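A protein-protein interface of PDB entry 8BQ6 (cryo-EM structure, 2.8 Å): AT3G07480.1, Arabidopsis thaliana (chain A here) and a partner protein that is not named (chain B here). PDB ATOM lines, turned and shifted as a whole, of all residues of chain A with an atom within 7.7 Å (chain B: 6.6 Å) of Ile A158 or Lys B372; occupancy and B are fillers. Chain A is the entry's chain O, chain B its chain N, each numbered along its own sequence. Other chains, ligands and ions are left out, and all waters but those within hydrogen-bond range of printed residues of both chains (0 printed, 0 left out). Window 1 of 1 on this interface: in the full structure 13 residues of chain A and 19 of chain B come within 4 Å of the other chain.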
ATOM      1  N   ALA A  81       8.677 -22.913 -23.414  1.00  0.00           N
ATOM      2  CA  ALA A  81       9.532 -22.321 -22.395  1.00  0.00           C
ATOM      3  C   ALA A  81       8.793 -21.303 -21.538  1.00  0.00           C
ATOM      4  O   ALA A  81       9.244 -20.998 -20.429  1.00  0.00           O
ATOM      5  CB  ALA A  81      10.746 -21.672 -23.055  1.00  0.00           C
ATOM      6  N   SER A  82       7.672 -20.779 -22.027  1.00  0.00           N
ATOM      7  CA  SER A  82       6.905 -19.775 -21.304  1.00  0.00           C
ATOM      8  C   SER A  82       5.935 -20.377 -20.299  1.00  0.00           C
ATOM      9  O   SER A  82       5.471 -19.662 -19.405  1.00  0.00           O
ATOM     10  CB  SER A  82       6.137 -18.908 -22.298  1.00  0.00           C
ATOM     11  OG  SER A  82       4.944 -19.553 -22.699  1.00  0.00           O
ATOM     12  N   ARG A  84       6.112 -24.033 -18.545  1.00  0.00           N
ATOM     13  CA  ARG A  84       6.706 -25.394 -18.442  1.00  0.00           C
ATOM     14  C   ARG A  84       5.873 -26.327 -17.558  1.00  0.00           C
ATOM     15  O   ARG A  84       5.962 -27.542 -17.779  1.00  0.00           O
ATOM     16  CB  ARG A  84       8.135 -25.269 -17.914  1.00  0.00           C
ATOM     17  CG  ARG A  84       9.105 -24.719 -18.948  1.00  0.00           C
ATOM     18  CD  ARG A  84      10.497 -24.486 -18.404  1.00  0.00           C
ATOM     19  NE  ARG A  84      10.530 -23.447 -17.387  1.00  0.00           N
ATOM     20  CZ  ARG A  84      11.592 -23.153 -16.647  1.00  0.00           C
ATOM     21  NH1 ARG A  84      12.720 -23.822 -16.810  1.00  0.00           N
ATOM     22  NH2 ARG A  84      11.522 -22.193 -15.745  1.00  0.00           N
ATOM     23  N   GLU A  89      -0.681 -22.545 -10.268  1.00  0.00           N
ATOM     24  CA  GLU A  89       0.212 -21.725  -9.461  1.00  0.00           C
ATOM     25  C   GLU A  89       1.457 -21.287 -10.221  1.00  0.00           C
ATOM     26  O   GLU A  89       2.263 -20.530  -9.671  1.00  0.00           O
ATOM     27  CB  GLU A  89       0.617 -22.484  -8.199  1.00  0.00           C
ATOM     28  CG  GLU A  89      -0.534 -23.215  -7.543  1.00  0.00           C
ATOM     29  CD  GLU A  89      -0.750 -22.797  -6.107  1.00  0.00           C
ATOM     30  OE1 GLU A  89      -0.469 -21.626  -5.777  1.00  0.00           O
ATOM     31  OE2 GLU A  89      -1.217 -23.639  -5.314  1.00  0.00           O
ATOM     32  N   ALA A  90       1.642 -21.749 -11.452  1.00  0.00           N
ATOM     33  CA  ALA A  90       2.743 -21.322 -12.302  1.00  0.00           C
ATOM     34  C   ALA A  90       2.215 -20.779 -13.620  1.00  0.00           C
ATOM     35  O   ALA A  90       2.735 -21.081 -14.696  1.00  0.00           O
ATOM     36  CB  ALA A  90       3.724 -22.467 -12.543  1.00  0.00           C
ATOM     37  N   CYS A  91       1.165 -19.969 -13.552  1.00  0.00           N
ATOM     38  CA  CYS A  91       0.473 -19.509 -14.742  1.00  0.00           C
ATOM     39  C   CYS A  91       0.169 -18.026 -14.611  1.00  0.00           C
ATOM     40  O   CYS A  91      -0.408 -17.593 -13.610  1.00  0.00           O
ATOM     41  CB  CYS A  91      -0.817 -20.303 -14.956  1.00  0.00           C
ATOM     42  SG  CYS A  91      -2.000 -19.536 -16.073  1.00  0.00           S
ATOM     43  N   SER A  92       0.567 -17.257 -15.618  1.00  0.00           N
ATOM     44  CA  SER A  92       0.179 -15.862 -15.758  1.00  0.00           C
ATOM     45  C   SER A  92      -0.565 -15.658 -17.069  1.00  0.00           C
ATOM     46  O   SER A  92      -0.342 -14.683 -17.789  1.00  0.00           O
ATOM     47  CB  SER A  92       1.390 -14.938 -15.672  1.00  0.00           C
ATOM     48  OG  SER A  92       2.041 -15.063 -14.423  1.00  0.00           O
ATOM     49  N   ALA A  93      -1.444 -16.603 -17.393  1.00  0.00           N
ATOM     50  CA  ALA A  93      -2.259 -16.594 -18.605  1.00  0.00           C
ATOM     51  C   ALA A  93      -1.421 -16.589 -19.880  1.00  0.00           C
ATOM     52  O   ALA A  93      -1.894 -16.154 -20.930  1.00  0.00           O
ATOM     53  CB  ALA A  93      -3.242 -15.419 -18.611  1.00  0.00           C
ATOM     54  N   GLU A  94      -0.183 -17.088 -19.819  1.00  0.00           N
ATOM     55  CA  GLU A  94       0.576 -17.323 -21.042  1.00  0.00           C
ATOM     56  C   GLU A  94      -0.048 -18.424 -21.884  1.00  0.00           C
ATOM     57  O   GLU A  94       0.266 -18.540 -23.072  1.00  0.00           O
ATOM     58  CB  GLU A  94       2.021 -17.695 -20.716  1.00  0.00           C
ATOM     59  CG  GLU A  94       2.786 -16.650 -19.938  1.00  0.00           C
ATOM     60  CD  GLU A  94       2.736 -16.894 -18.447  1.00  0.00           C
ATOM     61  OE1 GLU A  94       1.988 -17.797 -18.016  1.00  0.00           O
ATOM     62  OE2 GLU A  94       3.440 -16.185 -17.703  1.00  0.00           O
ATOM     63  N   PRO A 155       4.229 -10.899 -22.737  1.00  0.00           N
ATOM     64  CA  PRO A 155       5.612 -11.048 -22.281  1.00  0.00           C
ATOM     65  C   PRO A 155       5.655 -11.868 -21.006  1.00  0.00           C
ATOM     66  O   PRO A 155       4.822 -11.711 -20.110  1.00  0.00           O
ATOM     67  CB  PRO A 155       6.078  -9.606 -22.047  1.00  0.00           C
ATOM     68  CG  PRO A 155       5.005  -8.731 -22.605  1.00  0.00           C
ATOM     69  CD  PRO A 155       3.743  -9.524 -22.569  1.00  0.00           C
ATOM     70  N   TRP A 156       6.640 -12.751 -20.933  1.00  0.00           N
ATOM     71  CA  TRP A 156       6.691 -13.720 -19.849  1.00  0.00           C
ATOM     72  C   TRP A 156       8.054 -13.857 -19.200  1.00  0.00           C
ATOM     73  O   TRP A 156       8.132 -14.407 -18.097  1.00  0.00           O
ATOM     74  CB  TRP A 156       6.251 -15.093 -20.365  1.00  0.00           C
ATOM     75  CG  TRP A 156       7.146 -15.619 -21.435  1.00  0.00           C
ATOM     76  CD1 TRP A 156       6.997 -15.461 -22.779  1.00  0.00           C
ATOM     77  CD2 TRP A 156       8.333 -16.390 -21.251  1.00  0.00           C
ATOM     78  NE1 TRP A 156       8.021 -16.084 -23.445  1.00  0.00           N
ATOM     79  CE2 TRP A 156       8.855 -16.664 -22.526  1.00  0.00           C
ATOM     80  CE3 TRP A 156       9.005 -16.879 -20.128  1.00  0.00           C
ATOM     81  CZ2 TRP A 156      10.015 -17.402 -22.712  1.00  0.00           C
ATOM     82  CZ3 TRP A 156      10.154 -17.606 -20.313  1.00  0.00           C
ATOM     83  CH2 TRP A 156      10.649 -17.863 -21.595  1.00  0.00           C
ATOM     84  N   ASP A 157       9.112 -13.425 -19.889  1.00  0.00           N
ATOM     85  CA  ASP A 157      10.492 -13.640 -19.376  1.00  0.00           C
ATOM     86  C   ASP A 157      10.904 -12.468 -18.493  1.00  0.00           C
ATOM     87  O   ASP A 157      11.434 -11.481 -19.023  1.00  0.00           O
ATOM     88  CB  ASP A 157      11.481 -13.903 -20.511  1.00  0.00           C
ATOM     89  CG  ASP A 157      12.795 -14.525 -20.079  1.00  0.00           C
ATOM     90  OD1 ASP A 157      12.905 -14.947 -18.911  1.00  0.00           O
ATOM     91  OD2 ASP A 157      13.702 -14.583 -20.924  1.00  0.00           O
ATOM     92  N   ILE A 158      10.710 -12.615 -17.192  1.00  0.00           N
ATOM     93  CA  ILE A 158      11.051 -11.575 -16.226  1.00  0.00           C
ATOM     94  C   ILE A 158      12.568 -11.492 -16.092  1.00  0.00           C
ATOM     95  O   ILE A 158      13.223 -12.517 -15.854  1.00  0.00           O
ATOM     96  CB  ILE A 158      10.392 -11.837 -14.861  1.00  0.00           C
ATOM     97  CG1 ILE A 158       8.920 -11.395 -14.825  1.00  0.00           C
ATOM     98  CG2 ILE A 158      11.169 -11.146 -13.755  1.00  0.00           C
ATOM     99  CD1 ILE A 158       8.079 -11.742 -16.020  1.00  0.00           C
ATOM    100  N   PRO A 159      13.172 -10.303 -16.246  1.00  0.00           N
ATOM    101  CA  PRO A 159      14.616 -10.084 -16.115  1.00  0.00           C
ATOM    102  C   PRO A 159      15.176 -10.578 -14.785  1.00  0.00           C
ATOM    103  O   PRO A 159      14.575 -10.308 -13.747  1.00  0.00           O
ATOM    104  CB  PRO A 159      14.745  -8.566 -16.216  1.00  0.00           C
ATOM    105  CG  PRO A 159      13.600  -8.153 -17.039  1.00  0.00           C
ATOM    106  CD  PRO A 159      12.478  -9.096 -16.723  1.00  0.00           C
ATOM    107  N   GLU B 118      23.606 -15.345 -20.036  1.00  0.00           N
ATOM    108  CA  GLU B 118      22.562 -14.565 -20.740  1.00  0.00           C
ATOM    109  C   GLU B 118      23.233 -13.767 -21.840  1.00  0.00           C
ATOM    110  O   GLU B 118      22.510 -13.329 -22.746  1.00  0.00           O
ATOM    111  CB  GLU B 118      21.998 -13.548 -19.748  1.00  0.00           C
ATOM    112  CG  GLU B 118      20.724 -12.850 -20.173  1.00  0.00           C
ATOM    113  CD  GLU B 118      19.472 -13.658 -19.893  1.00  0.00           C
ATOM    114  OE1 GLU B 118      19.002 -13.641 -18.738  1.00  0.00           O
ATOM    115  OE2 GLU B 118      18.980 -14.308 -20.831  1.00  0.00           O
ATOM    116  N   SER B 169      13.431  -5.319 -23.182  1.00  0.00           N
ATOM    117  CA  SER B 169      12.460  -6.056 -22.393  1.00  0.00           C
ATOM    118  C   SER B 169      11.339  -5.126 -21.945  1.00  0.00           C
ATOM    119  O   SER B 169      11.592  -4.010 -21.488  1.00  0.00           O
ATOM    120  CB  SER B 169      13.145  -6.693 -21.185  1.00  0.00           C
ATOM    121  OG  SER B 169      12.238  -6.915 -20.124  1.00  0.00           O
ATOM    122  N   PHE B 171       9.464  -5.587 -19.369  1.00  0.00           N
ATOM    123  CA  PHE B 171       9.513  -5.485 -17.918  1.00  0.00           C
ATOM    124  C   PHE B 171      10.571  -4.492 -17.464  1.00  0.00           C
ATOM    125  O   PHE B 171      10.329  -3.678 -16.569  1.00  0.00           O
ATOM    126  CB  PHE B 171       9.772  -6.861 -17.318  1.00  0.00           C
ATOM    127  CG  PHE B 171       8.761  -7.877 -17.718  1.00  0.00           C
ATOM    128  CD1 PHE B 171       7.515  -7.887 -17.127  1.00  0.00           C
ATOM    129  CD2 PHE B 171       9.046  -8.813 -18.693  1.00  0.00           C
ATOM    130  CE1 PHE B 171       6.573  -8.815 -17.494  1.00  0.00           C
ATOM    131  CE2 PHE B 171       8.110  -9.745 -19.061  1.00  0.00           C
ATOM    132  CZ  PHE B 171       6.869  -9.743 -18.465  1.00  0.00           C
ATOM    133  N   TYR B 254      11.750  -4.126  -8.304  1.00  0.00           N
ATOM    134  CA  TYR B 254      12.521  -5.311  -7.952  1.00  0.00           C
ATOM    135  C   TYR B 254      12.250  -6.443  -8.925  1.00  0.00           C
ATOM    136  O   TYR B 254      13.169  -7.178  -9.299  1.00  0.00           O
ATOM    137  CB  TYR B 254      12.207  -5.771  -6.529  1.00  0.00           C
ATOM    138  CG  TYR B 254      12.799  -4.917  -5.439  1.00  0.00           C
ATOM    139  CD1 TYR B 254      13.337  -3.668  -5.714  1.00  0.00           C
ATOM    140  CD2 TYR B 254      12.859  -5.380  -4.139  1.00  0.00           C
ATOM    141  CE1 TYR B 254      13.882  -2.894  -4.716  1.00  0.00           C
ATOM    142  CE2 TYR B 254      13.408  -4.618  -3.139  1.00  0.00           C
ATOM    143  CZ  TYR B 254      13.918  -3.377  -3.432  1.00  0.00           C
ATOM    144  OH  TYR B 254      14.464  -2.618  -2.427  1.00  0.00           O
ATOM    145  N   GLU B 255      10.989  -6.614  -9.333  1.00  0.00           N
ATOM    146  CA  GLU B 255      10.681  -7.671 -10.288  1.00  0.00           C
ATOM    147  C   GLU B 255      11.223  -7.332 -11.670  1.00  0.00           C
ATOM    148  O   GLU B 255      11.838  -8.175 -12.334  1.00  0.00           O
ATOM    149  CB  GLU B 255       9.179  -7.868 -10.414  1.00  0.00           C
ATOM    150  CG  GLU B 255       8.861  -9.215 -10.993  1.00  0.00           C
ATOM    151  CD  GLU B 255       7.433  -9.593 -10.787  1.00  0.00           C
ATOM    152  OE1 GLU B 255       6.869  -9.130  -9.820  1.00  0.00           O
ATOM    153  OE2 GLU B 255       6.930 -10.469 -11.508  1.00  0.00           O
ATOM    154  N   GLY B 256      10.953  -6.110 -12.141  1.00  0.00           N
ATOM    155  CA  GLY B 256      11.220  -5.768 -13.522  1.00  0.00           C
ATOM    156  C   GLY B 256      12.678  -5.571 -13.853  1.00  0.00           C
ATOM    157  O   GLY B 256      13.065  -5.731 -15.012  1.00  0.00           O
ATOM    158  N   SER B 257      13.493  -5.229 -12.862  1.00  0.00           N
ATOM    159  CA  SER B 257      14.908  -5.035 -13.092  1.00  0.00           C
ATOM    160  C   SER B 257      15.613  -6.371 -13.299  1.00  0.00           C
ATOM    161  O   SER B 257      15.140  -7.416 -12.845  1.00  0.00           O
ATOM    162  CB  SER B 257      15.543  -4.295 -11.921  1.00  0.00           C
ATOM    163  OG  SER B 257      14.962  -3.018 -11.751  1.00  0.00           O
ATOM    164  N   THR B 259      17.971  -9.329 -12.466  1.00  0.00           N
ATOM    165  CA  THR B 259      18.113  -9.886 -11.122  1.00  0.00           C
ATOM    166  C   THR B 259      19.357  -9.422 -10.366  1.00  0.00           C
ATOM    167  O   THR B 259      19.247  -9.188  -9.152  1.00  0.00           O
ATOM    168  CB  THR B 259      18.058 -11.418 -11.201  1.00  0.00           C
ATOM    169  OG1 THR B 259      16.981 -11.803 -12.063  1.00  0.00           O
ATOM    170  CG2 THR B 259      17.817 -12.013  -9.820  1.00  0.00           C
ATOM    171  N   THR B 313       2.951 -15.371  -5.676  1.00  0.00           N
ATOM    172  CA  THR B 313       3.306 -16.667  -6.250  1.00  0.00           C
ATOM    173  C   THR B 313       4.651 -16.666  -6.965  1.00  0.00           C
ATOM    174  O   THR B 313       5.060 -17.713  -7.477  1.00  0.00           O
ATOM    175  CB  THR B 313       2.234 -17.154  -7.236  1.00  0.00           C
ATOM    176  OG1 THR B 313       2.124 -16.237  -8.333  1.00  0.00           O
ATOM    177  CG2 THR B 313       0.887 -17.299  -6.556  1.00  0.00           C
ATOM    178  N   LYS B 314       5.341 -15.532  -7.028  1.00  0.00           N
ATOM    179  CA  LYS B 314       6.629 -15.434  -7.694  1.00  0.00           C
ATOM    180  C   LYS B 314       7.714 -15.097  -6.682  1.00  0.00           C
ATOM    181  O   LYS B 314       7.495 -14.314  -5.753  1.00  0.00           O
ATOM    182  CB  LYS B 314       6.593 -14.390  -8.806  1.00  0.00           C
ATOM    183  CG  LYS B 314       5.631 -14.746  -9.908  1.00  0.00           C
ATOM    184  CD  LYS B 314       5.736 -13.797 -11.072  1.00  0.00           C
ATOM    185  CE  LYS B 314       4.631 -12.773 -11.022  1.00  0.00           C
ATOM    186  NZ  LYS B 314       4.794 -11.765 -12.092  1.00  0.00           N
ATOM    187  N   VAL B 315       8.890 -15.692  -6.881  1.00  0.00           N
ATOM    188  CA  VAL B 315       9.952 -15.625  -5.881  1.00  0.00           C
ATOM    189  C   VAL B 315      10.407 -14.184  -5.662  1.00  0.00           C
ATOM    190  O   VAL B 315      10.600 -13.742  -4.521  1.00  0.00           O
ATOM    191  CB  VAL B 315      11.128 -16.528  -6.294  1.00  0.00           C
ATOM    192  CG1 VAL B 315      12.222 -16.486  -5.242  1.00  0.00           C
ATOM    193  CG2 VAL B 315      10.649 -17.955  -6.517  1.00  0.00           C
ATOM    194  N   LYS B 316      10.594 -13.433  -6.750  1.00  0.00           N
ATOM    195  CA  LYS B 316      11.141 -12.086  -6.621  1.00  0.00           C
ATOM    196  C   LYS B 316      10.182 -11.157  -5.884  1.00  0.00           C
ATOM    197  O   LYS B 316      10.610 -10.346  -5.052  1.00  0.00           O
ATOM    198  CB  LYS B 316      11.494 -11.531  -7.999  1.00  0.00           C
ATOM    199  CG  LYS B 316      12.820 -12.041  -8.537  1.00  0.00           C
ATOM    200  CD  LYS B 316      13.109 -11.453  -9.896  1.00  0.00           C
ATOM    201  CE  LYS B 316      13.927 -10.192  -9.758  1.00  0.00           C
ATOM    202  NZ  LYS B 316      14.678  -9.851 -10.985  1.00  0.00           N
ATOM    203  N   LEU B 366      19.526 -20.117  -9.579  1.00  0.00           N
ATOM    204  CA  LEU B 366      18.371 -20.796 -10.234  1.00  0.00           C
ATOM    205  C   LEU B 366      17.924 -20.047 -11.497  1.00  0.00           C
ATOM    206  O   LEU B 366      17.149 -20.628 -12.267  1.00  0.00           O
ATOM    207  CB  LEU B 366      17.219 -20.925  -9.233  1.00  0.00           C
ATOM    208  CG  LEU B 366      17.513 -21.747  -7.980  1.00  0.00           C
ATOM    209  CD1 LEU B 366      16.423 -21.552  -6.942  1.00  0.00           C
ATOM    210  CD2 LEU B 366      17.678 -23.220  -8.308  1.00  0.00           C
ATOM    211  N   ARG B 367      18.416 -18.823 -11.719  1.00  0.00           N
ATOM    212  CA  ARG B 367      17.990 -18.007 -12.887  1.00  0.00           C
ATOM    213  C   ARG B 367      18.633 -18.555 -14.163  1.00  0.00           C
ATOM    214  O   ARG B 367      18.167 -18.178 -15.248  1.00  0.00           O
ATOM    215  CB  ARG B 367      18.300 -16.528 -12.649  1.00  0.00           C
ATOM    216  CG  ARG B 367      17.099 -15.719 -12.184  1.00  0.00           C
ATOM    217  CD  ARG B 367      16.166 -15.402 -13.335  1.00  0.00           C
ATOM    218  NE  ARG B 367      16.811 -14.576 -14.344  1.00  0.00           N
ATOM    219  CZ  ARG B 367      16.258 -14.224 -15.499  1.00  0.00           C
ATOM    220  NH1 ARG B 367      15.038 -14.632 -15.801  1.00  0.00           N
ATOM    221  NH2 ARG B 367      16.928 -13.468 -16.350  1.00  0.00           N
ATOM    222  N   THR B 369      18.240 -21.563 -15.074  1.00  0.00           N
ATOM    223  CA  THR B 369      17.133 -22.390 -15.640  1.00  0.00           C
ATOM    224  C   THR B 369      15.842 -21.563 -15.551  1.00  0.00           C
ATOM    225  O   THR B 369      14.764 -22.172 -15.545  1.00  0.00           O
ATOM    226  CB  THR B 369      17.115 -23.809 -15.056  1.00  0.00           C
ATOM    227  OG1 THR B 369      18.347 -24.456 -15.377  1.00  0.00           O
ATOM    228  CG2 THR B 369      15.971 -24.643 -15.588  1.00  0.00           C
ATOM    229  N   ARG B 370      15.952 -20.239 -15.418  1.00  0.00           N
ATOM    230  CA  ARG B 370      14.787 -19.302 -15.470  1.00  0.00           C
ATOM    231  C   ARG B 370      13.728 -19.549 -14.388  1.00  0.00           C
ATOM    232  O   ARG B 370      12.541 -19.591 -14.751  1.00  0.00           O
ATOM    233  CB  ARG B 370      14.175 -19.325 -16.874  1.00  0.00           C
ATOM    234  CG  ARG B 370      15.121 -18.860 -17.966  1.00  0.00           C
ATOM    235  CD  ARG B 370      15.632 -17.490 -17.589  1.00  0.00           C
ATOM    236  NE  ARG B 370      15.546 -16.575 -18.709  1.00  0.00           N
ATOM    237  CZ  ARG B 370      16.594 -16.138 -19.388  1.00  0.00           C
ATOM    238  NH1 ARG B 370      17.810 -16.534 -19.053  1.00  0.00           N
ATOM    239  NH2 ARG B 370      16.422 -15.308 -20.399  1.00  0.00           N
ATOM    240  N   VAL B 371      14.118 -19.648 -13.118  1.00  0.00           N
ATOM    241  CA  VAL B 371      13.105 -19.738 -12.022  1.00  0.00           C
ATOM    242  C   VAL B 371      12.237 -18.469 -12.054  1.00  0.00           C
ATOM    243  O   VAL B 371      12.775 -17.365 -12.262  1.00  0.00           O
ATOM    244  CB  VAL B 371      13.762 -19.966 -10.641  1.00  0.00           C
ATOM    245  CG1 VAL B 371      14.508 -18.749 -10.112  1.00  0.00           C
ATOM    246  CG2 VAL B 371      12.767 -20.480  -9.611  1.00  0.00           C
ATOM    247  N   LYS B 372      10.927 -18.622 -11.905  1.00  0.00           N
ATOM    248  CA  LYS B 372       9.995 -17.464 -11.898  1.00  0.00           C
ATOM    249  C   LYS B 372       8.956 -17.677 -10.799  1.00  0.00           C
ATOM    250  O   LYS B 372       8.704 -16.724 -10.055  1.00  0.00           O
ATOM    251  CB  LYS B 372       9.308 -17.336 -13.258  1.00  0.00           C
ATOM    252  CG  LYS B 372       8.502 -16.065 -13.475  1.00  0.00           C
ATOM    253  CD  LYS B 372       7.800 -16.044 -14.809  1.00  0.00           C
ATOM    254  CE  LYS B 372       6.622 -15.097 -14.852  1.00  0.00           C
ATOM    255  NZ  LYS B 372       5.942 -15.143 -16.167  1.00  0.00           N
ATOM    256  N   TYR B 373       8.427 -18.893 -10.670  1.00  0.00           N
ATOM    257  CA  TYR B 373       7.357 -19.148  -9.721  1.00  0.00           C
ATOM    258  C   TYR B 373       7.865 -19.964  -8.541  1.00  0.00           C
ATOM    259  O   TYR B 373       8.872 -20.669  -8.635  1.00  0.00           O
ATOM    260  CB  TYR B 373       6.201 -19.893 -10.386  1.00  0.00           C
ATOM    261  CG  TYR B 373       5.551 -19.149 -11.525  1.00  0.00           C
ATOM    262  CD1 TYR B 373       4.604 -18.166 -11.286  1.00  0.00           C
ATOM    263  CD2 TYR B 373       5.878 -19.438 -12.840  1.00  0.00           C
ATOM    264  CE1 TYR B 373       4.006 -17.488 -12.324  1.00  0.00           C
ATOM    265  CE2 TYR B 373       5.285 -18.769 -13.880  1.00  0.00           C
ATOM    266  CZ  TYR B 373       4.352 -17.794 -13.618  1.00  0.00           C
ATOM    267  OH  TYR B 373       3.759 -17.127 -14.662  1.00  0.00           O
ATOM    268  N   ILE B 374       7.143 -19.860  -7.424  1.00  0.00           N
ATOM    269  CA  ILE B 374       7.442 -20.687  -6.258  1.00  0.00           C
ATOM    270  C   ILE B 374       7.237 -22.161  -6.584  1.00  0.00           C
ATOM    271  O   ILE B 374       7.936 -23.033  -6.055  1.00  0.00           O
ATOM    272  CB  ILE B 374       6.585 -20.234  -5.062  1.00  0.00           C
ATOM    273  CG1 ILE B 374       7.046 -18.856  -4.586  1.00  0.00           C
ATOM    274  CG2 ILE B 374       6.626 -21.252  -3.926  1.00  0.00           C
ATOM    275  CD1 ILE B 374       5.975 -18.061  -3.907  1.00  0.00           C
ATOM    276  N   ALA B 375       6.289 -22.463  -7.473  1.00  0.00           N
ATOM    277  CA  ALA B 375       6.035 -23.849  -7.841  1.00  0.00           C
ATOM    278  C   ALA B 375       7.168 -24.449  -8.665  1.00  0.00           C
ATOM    279  O   ALA B 375       7.290 -25.676  -8.725  1.00  0.00           O
ATOM    280  CB  ALA B 375       4.714 -23.955  -8.600  1.00  0.00           C
ATOM    281  N   ASP B 376       7.992 -23.618  -9.298  1.00  0.00           N
ATOM    282  CA  ASP B 376       9.162 -24.127 -10.063  1.00  0.00           C
ATOM    283  C   ASP B 376      10.138 -24.850  -9.128  1.00  0.00           C
ATOM    284  O   ASP B 376      10.919 -25.669  -9.630  1.00  0.00           O
ATOM    285  CB  ASP B 376       9.842 -22.990 -10.825  1.00  0.00           C
ATOM    286  CG  ASP B 376       8.987 -22.350 -11.906  1.00  0.00           C
ATOM    287  OD1 ASP B 376       7.853 -22.823 -12.124  1.00  0.00           O
ATOM    288  OD2 ASP B 376       9.467 -21.380 -12.531  1.00  0.00           O
ATOM    289  N   TYR B 458      17.717 -28.066 -12.650  1.00  0.00           N
ATOM    290  CA  TYR B 458      18.450 -26.812 -12.616  1.00  0.00           C
ATOM    291  C   TYR B 458      19.933 -27.068 -12.830  1.00  0.00           C
ATOM    292  O   TYR B 458      20.476 -28.073 -12.364  1.00  0.00           O
ATOM    293  CB  TYR B 458      18.232 -26.089 -11.286  1.00  0.00           C
ATOM    294  CG  TYR B 458      16.821 -25.593 -11.102  1.00  0.00           C
ATOM    295  CD1 TYR B 458      16.432 -24.366 -11.610  1.00  0.00           C
ATOM    296  CD2 TYR B 458      15.878 -26.347 -10.410  1.00  0.00           C
ATOM    297  CE1 TYR B 458      15.151 -23.907 -11.454  1.00  0.00           C
ATOM    298  CE2 TYR B 458      14.588 -25.890 -10.244  1.00  0.00           C
ATOM    299  CZ  TYR B 458      14.233 -24.667 -10.769  1.00  0.00           C
ATOM    300  OH  TYR B 458      12.955 -24.188 -10.618  1.00  0.00           O
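Among the printed residues, merely in contact across the chains: Glu A89 with Tyr B373, Ala A90 with Tyr B373, Cys A91 with Tyr B373, Pro A155 with Phe B171, Trp A156 with Phe B171, Asp A157 with Phe B171, Ile A158 with Phe B171, Ile A158 with Glu B255, Ile A158 with Lys B372, Pro A159 with Ser B169, Pro A159 with Phe B171, Pro A159 with Glu B255, Pro A159 with Gly B256 and Pro A159 with Arg B367.
The side-chain amino group (NZ) of Lys B316 is in hydrogen-bond range of the backbone carbonyl oxygen (O) of Pro A159, at 2.8 Å. The side-chain carboxylate (OD2) of Asp B376 lies within salt-bridge range of the guanidinium group (NH2) of Arg A84, 3.9 Å away. The backbone carbonyl oxygen of Thr B369 sits at hydrogen-bond distance from the guanidinium group of Arg A84 (2.9 Å). The guanidinium group (NH2) of Arg A84 sits at hydrogen-bond distance from the backbone carbonyl oxygen (O) of Arg B370 (3.0 Å). O of Pro A159 lies close to O of Ser B257 (3.1 Å). OG1 of Thr B259 sits at hydrogen-bond distance from O of Pro A159 (3.3 Å). The backbone carbonyl oxygen of Ile A158 lies within hydrogen-bond range of the guanidinium group of Arg B367, at 2.8 Å. OH of Tyr B373 is in hydrogen-bond range of OG of Ser A92 (2.7 Å). The backbone carbonyl oxygen of Trp A156 lies within hydrogen-bond range of the side-chain amino group of Lys B372 (3.0 Å). The side-chain carboxylate (OD1) of Asp A157 lies within salt-bridge range of the guanidinium group (NH1) of Arg B367 (3.8 Å). OE2 of Glu A94 lies within hydrogen-bond range of OH of Tyr B373 (3.2 Å). The side-chain carboxylate (OE2) of Glu A94 is in salt-bridge range of the side-chain amino group (NZ) of Lys B372, at 3.1 Å. NH2 of Arg B370 lies within salt-bridge range of OD2 of Asp A157 (2.9 Å).
Of the printed residues of chain B, Asp A157 touches Phe B171 (3.6 Å), Arg B367 (3.8 Å) and Arg B370 (2.9 Å). Lys B372 touches just these residues of chain A: Glu A94 (3.1 Å), Trp A156 (3.0 Å) and Ile A158 (3.8 Å). Of the printed residues of chain A, Tyr B373 touches Glu A89 (3.7 Å), Ala A90 (3.5 Å), Cys A91 (3.7 Å), Ser A92 (2.7 Å) and Glu A94 (3.2 Å). The nearest residue of chain B that does not touch Ile A158 is Lys B316 (4.3 Å). The nearest residue of chain A that does not touch Lys B372 is Ser A92 (4.3 Å).
O of Asp B376 lies within hydrogen-bond range of OH of Tyr B458 (2.7 Å). The side-chain hydroxyl (OG1) of Thr B259 sits at hydrogen-bond distance from the side-chain amino group (NZ) of Lys B316 (3.2 Å). The backbone carbonyl oxygen of Lys B372 is in hydrogen-bond range of the backbone NH of Val B315 (3.3 Å). OE1 of Glu B118 lies within salt-bridge range of NH2 of Arg B367, at 3.2 Å. The backbone NH (N) of Tyr B373 lies within hydrogen-bond range of the side-chain carboxylate (OD2) of Asp B376, 3.3 Å away. The side-chain carboxylate (OE2) of Glu B118 lies within salt-bridge range of the guanidinium group (NH2) of Arg B370.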
